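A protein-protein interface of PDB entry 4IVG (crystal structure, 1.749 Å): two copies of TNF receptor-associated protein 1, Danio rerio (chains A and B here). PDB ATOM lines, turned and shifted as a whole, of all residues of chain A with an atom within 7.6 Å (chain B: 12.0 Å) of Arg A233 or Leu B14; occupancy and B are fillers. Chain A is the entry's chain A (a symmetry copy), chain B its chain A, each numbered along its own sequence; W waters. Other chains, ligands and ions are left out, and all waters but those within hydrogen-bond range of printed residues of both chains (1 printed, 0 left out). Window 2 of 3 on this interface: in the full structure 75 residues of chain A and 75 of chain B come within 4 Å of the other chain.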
ATOM      1  N   ILE A  86     -21.088  10.124  -9.448  1.00  0.00           N
ATOM      2  CA  ILE A  86     -21.956   9.844  -8.314  1.00  0.00           C
ATOM      3  C   ILE A  86     -21.129  10.002  -7.043  1.00  0.00           C
ATOM      4  O   ILE A  86     -20.090   9.339  -6.891  1.00  0.00           O
ATOM      5  CB  ILE A  86     -22.509   8.408  -8.381  1.00  0.00           C
ATOM      6  CG1 ILE A  86     -23.356   8.241  -9.651  1.00  0.00           C
ATOM      7  CG2 ILE A  86     -23.309   8.094  -7.131  1.00  0.00           C
ATOM      8  CD1 ILE A  86     -23.732   6.788  -9.980  1.00  0.00           C
ATOM      9  N   HIS A  87     -21.575  10.883  -6.138  1.00  0.00           N
ATOM     10  CA  HIS A  87     -20.873  11.092  -4.858  1.00  0.00           C
ATOM     11  C   HIS A  87     -21.705  10.637  -3.665  1.00  0.00           C
ATOM     12  O   HIS A  87     -22.923  10.845  -3.629  1.00  0.00           O
ATOM     13  CB  HIS A  87     -20.476  12.563  -4.691  1.00  0.00           C
ATOM     14  CG  HIS A  87     -19.375  12.993  -5.599  1.00  0.00           C
ATOM     15  ND1 HIS A  87     -18.088  13.193  -5.160  1.00  0.00           N
ATOM     16  CD2 HIS A  87     -19.364  13.253  -6.926  1.00  0.00           C
ATOM     17  CE1 HIS A  87     -17.330  13.559  -6.180  1.00  0.00           C
ATOM     18  NE2 HIS A  87     -18.081  13.602  -7.263  1.00  0.00           N
ATOM     19  N   LEU A  88     -21.037  10.010  -2.695  1.00  0.00           N
ATOM     20  CA  LEU A  88     -21.663   9.545  -1.461  1.00  0.00           C
ATOM     21  C   LEU A  88     -20.947  10.263  -0.332  1.00  0.00           C
ATOM     22  O   LEU A  88     -19.731  10.500  -0.409  1.00  0.00           O
ATOM     23  CB  LEU A  88     -21.472   8.039  -1.268  1.00  0.00           C
ATOM     24  CG  LEU A  88     -21.944   7.143  -2.421  1.00  0.00           C
ATOM     25  CD1 LEU A  88     -21.734   5.657  -2.058  1.00  0.00           C
ATOM     26  CD2 LEU A  88     -23.392   7.399  -2.752  1.00  0.00           C
ATOM     27  N   GLU A 210     -18.432   4.975   7.039  1.00  0.00           N
ATOM     28  CA  GLU A 210     -17.738   4.857   5.756  1.00  0.00           C
ATOM     29  C   GLU A 210     -17.440   3.416   5.338  1.00  0.00           C
ATOM     30  O   GLU A 210     -17.737   3.013   4.209  1.00  0.00           O
ATOM     31  CB  GLU A 210     -16.443   5.660   5.795  1.00  0.00           C
ATOM     32  CG  GLU A 210     -15.637   5.656   4.520  1.00  0.00           C
ATOM     33  CD  GLU A 210     -14.415   6.554   4.634  1.00  0.00           C
ATOM     34  OE1 GLU A 210     -13.320   6.050   4.957  1.00  0.00           O
ATOM     35  OE2 GLU A 210     -14.551   7.776   4.430  1.00  0.00           O
ATOM     36  N   ASP A 211     -16.851   2.634   6.239  1.00  0.00           N
ATOM     37  CA  ASP A 211     -16.556   1.236   5.900  1.00  0.00           C
ATOM     38  C   ASP A 211     -17.804   0.448   5.529  1.00  0.00           C
ATOM     39  O   ASP A 211     -17.781  -0.373   4.604  1.00  0.00           O
ATOM     40  CB  ASP A 211     -15.796   0.547   7.036  1.00  0.00           C
ATOM     41  CG  ASP A 211     -14.352   1.015   7.144  1.00  0.00           C
ATOM     42  OD1 ASP A 211     -13.850   1.650   6.191  1.00  0.00           O
ATOM     43  OD2 ASP A 211     -13.710   0.731   8.179  1.00  0.00           O
ATOM     44  N   LYS A 214     -18.974   1.439   2.017  1.00  0.00           N
ATOM     45  CA  LYS A 214     -18.033   0.867   1.070  1.00  0.00           C
ATOM     46  C   LYS A 214     -18.340  -0.597   0.775  1.00  0.00           C
ATOM     47  O   LYS A 214     -18.326  -1.002  -0.389  1.00  0.00           O
ATOM     48  CB  LYS A 214     -16.589   1.032   1.567  1.00  0.00           C
ATOM     49  CG  LYS A 214     -15.559   0.752   0.480  1.00  0.00           C
ATOM     50  CD  LYS A 214     -14.135   0.861   0.994  1.00  0.00           C
ATOM     51  CE  LYS A 214     -13.924   2.145   1.756  1.00  0.00           C
ATOM     52  NZ  LYS A 214     -12.483   2.346   2.046  1.00  0.00           N
ATOM     53  N   ILE A 228     -17.923   6.434  -8.889  1.00  0.00           N
ATOM     54  CA  ILE A 228     -18.570   6.606  -7.589  1.00  0.00           C
ATOM     55  C   ILE A 228     -17.493   7.015  -6.597  1.00  0.00           C
ATOM     56  O   ILE A 228     -16.452   6.362  -6.510  1.00  0.00           O
ATOM     57  CB  ILE A 228     -19.223   5.300  -7.113  1.00  0.00           C
ATOM     58  CG1 ILE A 228     -20.376   4.927  -8.044  1.00  0.00           C
ATOM     59  CG2 ILE A 228     -19.745   5.427  -5.672  1.00  0.00           C
ATOM     60  CD1 ILE A 228     -20.870   3.498  -7.848  1.00  0.00           C
ATOM     61  N   PHE A 229     -17.734   8.105  -5.868  1.00  0.00           N
ATOM     62  CA  PHE A 229     -16.799   8.563  -4.842  1.00  0.00           C
ATOM     63  C   PHE A 229     -17.482   8.484  -3.487  1.00  0.00           C
ATOM     64  O   PHE A 229     -18.685   8.725  -3.369  1.00  0.00           O
ATOM     65  CB  PHE A 229     -16.384  10.008  -5.123  1.00  0.00           C
ATOM     66  CG  PHE A 229     -15.646  10.187  -6.410  1.00  0.00           C
ATOM     67  CD1 PHE A 229     -16.333  10.385  -7.604  1.00  0.00           C
ATOM     68  CD2 PHE A 229     -14.267  10.163  -6.439  1.00  0.00           C
ATOM     69  CE1 PHE A 229     -15.646  10.557  -8.795  1.00  0.00           C
ATOM     70  CE2 PHE A 229     -13.581  10.335  -7.631  1.00  0.00           C
ATOM     71  CZ  PHE A 229     -14.274  10.529  -8.804  1.00  0.00           C
ATOM     72  N   LEU A 230     -16.723   8.134  -2.456  1.00  0.00           N
ATOM     73  CA  LEU A 230     -17.267   8.123  -1.109  1.00  0.00           C
ATOM     74  C   LEU A 230     -16.378   9.014  -0.236  1.00  0.00           C
ATOM     75  O   LEU A 230     -15.172   8.761  -0.082  1.00  0.00           O
ATOM     76  CB  LEU A 230     -17.340   6.686  -0.579  1.00  0.00           C
ATOM     77  CG  LEU A 230     -17.635   6.524   0.920  1.00  0.00           C
ATOM     78  CD1 LEU A 230     -19.031   7.049   1.268  1.00  0.00           C
ATOM     79  CD2 LEU A 230     -17.477   5.068   1.351  1.00  0.00           C
ATOM     80  N   ASN A 231     -16.966  10.093   0.278  1.00  0.00           N
ATOM     81  CA  ASN A 231     -16.206  11.086   1.034  1.00  0.00           C
ATOM     82  C   ASN A 231     -14.940  11.509   0.289  1.00  0.00           C
ATOM     83  O   ASN A 231     -13.878  11.716   0.886  1.00  0.00           O
ATOM     84  CB  ASN A 231     -15.868  10.527   2.423  1.00  0.00           C
ATOM     85  CG  ASN A 231     -17.102  10.167   3.213  1.00  0.00           C
ATOM     86  OD1 ASN A 231     -18.127  10.865   3.136  1.00  0.00           O
ATOM     87  ND2 ASN A 231     -17.034   9.058   3.954  1.00  0.00           N
ATOM     88  N   GLY A 232     -15.059  11.617  -1.035  1.00  0.00           N
ATOM     89  CA  GLY A 232     -13.962  12.085  -1.870  1.00  0.00           C
ATOM     90  C   GLY A 232     -13.061  11.016  -2.459  1.00  0.00           C
ATOM     91  O   GLY A 232     -12.194  11.334  -3.272  1.00  0.00           O
ATOM     92  N   ARG A 233     -13.247   9.766  -2.055  1.00  0.00           N
ATOM     93  CA  ARG A 233     -12.390   8.683  -2.546  1.00  0.00           C
ATOM     94  C   ARG A 233     -13.086   7.808  -3.579  1.00  0.00           C
ATOM     95  O   ARG A 233     -14.187   7.293  -3.339  1.00  0.00           O
ATOM     96  CB  ARG A 233     -11.902   7.811  -1.389  1.00  0.00           C
ATOM     97  CG  ARG A 233     -10.955   8.526  -0.453  1.00  0.00           C
ATOM     98  CD  ARG A 233     -10.409   7.572   0.584  1.00  0.00           C
ATOM     99  NE  ARG A 233     -10.164   8.252   1.850  1.00  0.00           N
ATOM    100  CZ  ARG A 233     -10.365   7.699   3.040  1.00  0.00           C
ATOM    101  NH1 ARG A 233     -10.812   6.451   3.124  1.00  0.00           N
ATOM    102  NH2 ARG A 233     -10.122   8.389   4.146  1.00  0.00           N
ATOM    103  N   ARG A 234     -12.430   7.630  -4.724  1.00  0.00           N
ATOM    104  CA  ARG A 234     -12.960   6.790  -5.804  1.00  0.00           C
ATOM    105  C   ARG A 234     -13.084   5.345  -5.336  1.00  0.00           C
ATOM    106  O   ARG A 234     -12.117   4.765  -4.835  1.00  0.00           O
ATOM    107  CB  ARG A 234     -12.039   6.864  -7.026  1.00  0.00           C
ATOM    108  CG  ARG A 234     -12.457   5.959  -8.186  1.00  0.00           C
ATOM    109  CD  ARG A 234     -13.710   6.477  -8.889  1.00  0.00           C
ATOM    110  NE  ARG A 234     -14.022   5.675 -10.074  1.00  0.00           N
ATOM    111  CZ  ARG A 234     -13.489   5.874 -11.276  1.00  0.00           C
ATOM    112  NH1 ARG A 234     -12.618   6.858 -11.458  1.00  0.00           N
ATOM    113  NH2 ARG A 234     -13.821   5.092 -12.295  1.00  0.00           N
ATOM    114  N   LEU A 235     -14.273   4.763  -5.495  1.00  0.00           N
ATOM    115  CA  LEU A 235     -14.505   3.386  -5.051  1.00  0.00           C
ATOM    116  C   LEU A 235     -14.442   2.342  -6.157  1.00  0.00           C
ATOM    117  O   LEU A 235     -14.139   1.181  -5.891  1.00  0.00           O
ATOM    118  CB  LEU A 235     -15.876   3.254  -4.401  1.00  0.00           C
ATOM    119  CG  LEU A 235     -16.110   4.015  -3.102  1.00  0.00           C
ATOM    120  CD1 LEU A 235     -17.433   3.531  -2.519  1.00  0.00           C
ATOM    121  CD2 LEU A 235     -14.956   3.772  -2.133  1.00  0.00           C
ATOM    122  N   ASN A 236     -14.779   2.734  -7.383  1.00  0.00           N
ATOM    123  CA  ASN A 236     -15.020   1.749  -8.446  1.00  0.00           C
ATOM    124  C   ASN A 236     -14.126   1.947  -9.672  1.00  0.00           C
ATOM    125  O   ASN A 236     -14.603   2.195 -10.783  1.00  0.00           O
ATOM    126  CB  ASN A 236     -16.505   1.748  -8.838  1.00  0.00           C
ATOM    127  CG  ASN A 236     -16.935   3.039  -9.522  1.00  0.00           C
ATOM    128  OD1 ASN A 236     -16.281   4.071  -9.374  1.00  0.00           O
ATOM    129  ND2 ASN A 236     -18.014   2.977 -10.307  1.00  0.00           N
ATOM    130  N   THR B  13      -5.800  14.096  -2.316  1.00  0.00           N
ATOM    131  CA  THR B  13      -6.196  13.597  -3.627  1.00  0.00           C
ATOM    132  C   THR B  13      -7.709  13.681  -3.744  1.00  0.00           C
ATOM    133  O   THR B  13      -8.274  13.479  -4.819  1.00  0.00           O
ATOM    134  CB  THR B  13      -5.746  12.131  -3.837  1.00  0.00           C
ATOM    135  OG1 THR B  13      -4.388  11.977  -3.408  1.00  0.00           O
ATOM    136  CG2 THR B  13      -5.859  11.722  -5.307  1.00  0.00           C
ATOM    137  N   LEU B  14      -8.355  14.003  -2.628  1.00  0.00           N
ATOM    138  CA  LEU B  14      -9.807  13.955  -2.531  1.00  0.00           C
ATOM    139  C   LEU B  14     -10.502  14.764  -3.607  1.00  0.00           C
ATOM    140  O   LEU B  14      -9.988  15.774  -4.096  1.00  0.00           O
ATOM    141  CB  LEU B  14     -10.283  14.414  -1.156  1.00  0.00           C
ATOM    142  CG  LEU B  14      -9.805  13.547   0.001  1.00  0.00           C
ATOM    143  CD1 LEU B  14     -10.325  14.106   1.314  1.00  0.00           C
ATOM    144  CD2 LEU B  14     -10.241  12.097  -0.188  1.00  0.00           C
ATOM    145  N   HIS B  15     -11.685  14.293  -3.968  1.00  0.00           N
ATOM    146  CA  HIS B  15     -12.482  14.918  -4.992  1.00  0.00           C
ATOM    147  C   HIS B  15     -13.931  14.838  -4.555  1.00  0.00           C
ATOM    148  O   HIS B  15     -14.573  13.798  -4.686  1.00  0.00           O
ATOM    149  CB  HIS B  15     -12.287  14.194  -6.317  1.00  0.00           C
ATOM    150  CG  HIS B  15     -13.118  14.745  -7.423  1.00  0.00           C
ATOM    151  ND1 HIS B  15     -13.901  13.955  -8.230  1.00  0.00           N
ATOM    152  CD2 HIS B  15     -13.314  16.018  -7.836  1.00  0.00           C
ATOM    153  CE1 HIS B  15     -14.532  14.717  -9.104  1.00  0.00           C
ATOM    154  NE2 HIS B  15     -14.194  15.974  -8.887  1.00  0.00           N
ATOM    155  N   ASN B  16     -14.436  15.933  -4.002  1.00  0.00           N
ATOM    156  CA  ASN B  16     -15.809  15.994  -3.544  1.00  0.00           C
ATOM    157  C   ASN B  16     -16.582  17.034  -4.327  1.00  0.00           C
ATOM    158  O   ASN B  16     -15.996  17.911  -4.972  1.00  0.00           O
ATOM    159  CB  ASN B  16     -15.860  16.342  -2.053  1.00  0.00           C
ATOM    160  CG  ASN B  16     -15.862  15.117  -1.163  1.00  0.00           C
ATOM    161  OD1 ASN B  16     -16.175  14.015  -1.608  1.00  0.00           O
ATOM    162  ND2 ASN B  16     -15.548  15.312   0.114  1.00  0.00           N
ATOM    163  N   ILE B  17     -17.902  16.929  -4.284  1.00  0.00           N
ATOM    164  CA  ILE B  17     -18.759  17.980  -4.793  1.00  0.00           C
ATOM    165  C   ILE B  17     -19.866  18.235  -3.783  1.00  0.00           C
ATOM    166  O   ILE B  17     -20.590  19.230  -3.890  1.00  0.00           O
ATOM    167  CB  ILE B  17     -19.375  17.619  -6.157  1.00  0.00           C
ATOM    168  CG1 ILE B  17     -20.366  16.473  -5.999  1.00  0.00           C
ATOM    169  CG2 ILE B  17     -18.290  17.278  -7.172  1.00  0.00           C
ATOM    170  CD1 ILE B  17     -21.251  16.266  -7.196  1.00  0.00           C
ATOM    171  N   ILE B  18     -20.001  17.337  -2.804  1.00  0.00           N
ATOM    172  CA  ILE B  18     -21.064  17.480  -1.813  1.00  0.00           C
ATOM    173  C   ILE B  18     -20.750  18.628  -0.862  1.00  0.00           C
ATOM    174  O   ILE B  18     -19.755  18.615  -0.130  1.00  0.00           O
ATOM    175  CB  ILE B  18     -21.380  16.183  -1.052  1.00  0.00           C
ATOM    176  CG1 ILE B  18     -21.823  15.111  -2.056  1.00  0.00           C
ATOM    177  CG2 ILE B  18     -22.482  16.440  -0.033  1.00  0.00           C
ATOM    178  CD1 ILE B  18     -22.303  13.794  -1.434  1.00  0.00           C
HETATM  179  O   HOH W   1     -17.648  12.000  -2.555  1.00  0.00           O
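The backbone NH (N) of Gly A232 lies within hydrogen-bond range of the side-chain amide oxygen (OD1) of Asn B16, 2.7 Å away. O of Gly A232 sits at hydrogen-bond distance from N of His B15 (3.1 Å).
Arg A233 touches just one residue of chain B: Leu B14. Leu B14 touches just these residues of chain A: Asn A231, Gly A232 and Arg A233. No residue of chain B comes within 4 Å of Leu A230. Of chain B, only Leu B14 and Asn B16 come within 4 Å of Asn A231. Gly A232 touches just these residues of chain B: Leu B14, His B15 and Asn B16. No residue of chain B comes within 4 Å of Leu A235. Printed residues of chain A within 4 Å of Ile B18: His A87 (3.7 Å) and Leu A88 (3.9 Å). Printed residues of chain A within 4 Å of His B15: His A87, Phe A229 and Gly A232. The nearest residue of chain B that does not touch Arg A233 is His B15 (5.0 Å). The nearest residue of chain A that does not touch Leu B14 is Leu A230 (6.0 Å).
Among the printed residues, pairs that only touch across the chains: His A87 with His B15, Asn A231 with Asn B16, Phe A229 with His B15, His A87 with Ile B17, Gly A232 with Leu B14, Arg A233 with Leu B14, His A87 with Ile B18, Asn A231 with Leu B14, His A87 with Asn B16 and Leu A88 with Ile B18.
Of the 6 printed residues of chain B, 5 touch a printed residue of chain A. Hydrophobic or aromatic side chains of chain B within 4 Å of the printed part of chain A: Leu B14, His B15, Ile B17 and Ile B18. Hydrophobic or aromatic side chains of chain A within 4 Å of the printed part of chain B: His A87 and Phe A229.
The backbone carbonyl oxygen (O) of Phe A229 sits at hydrogen-bond distance from the backbone NH (N) of Leu A88 (2.8 Å). OE1 of Glu A210 is in salt-bridge range of NH1 of Arg A233 (3.1 Å). N of Phe A229 lies within hydrogen-bond range of O of Ile A86 (2.8 Å). OE2 of Glu A210 sits at hydrogen-bond distance from ND2 of Asn A231 (2.8 Å). The backbone carbonyl oxygen of Leu A88 sits at hydrogen-bond distance from the backbone NH of Asn A231.
No position is printed for both chains. Of the 12 pairs that touch across the chains among the printed residues, none has its exchanged pair printed and touching as well.
Water W1 lies within hydrogen-bond range of OD1 of Asn B16 (2.7 Å), ND1 of His A87 (2.9 Å), N of Gly A232 (3.0 Å), O of Leu A88 (3.3 Å) and N of Asn A231 (3.5 Å).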
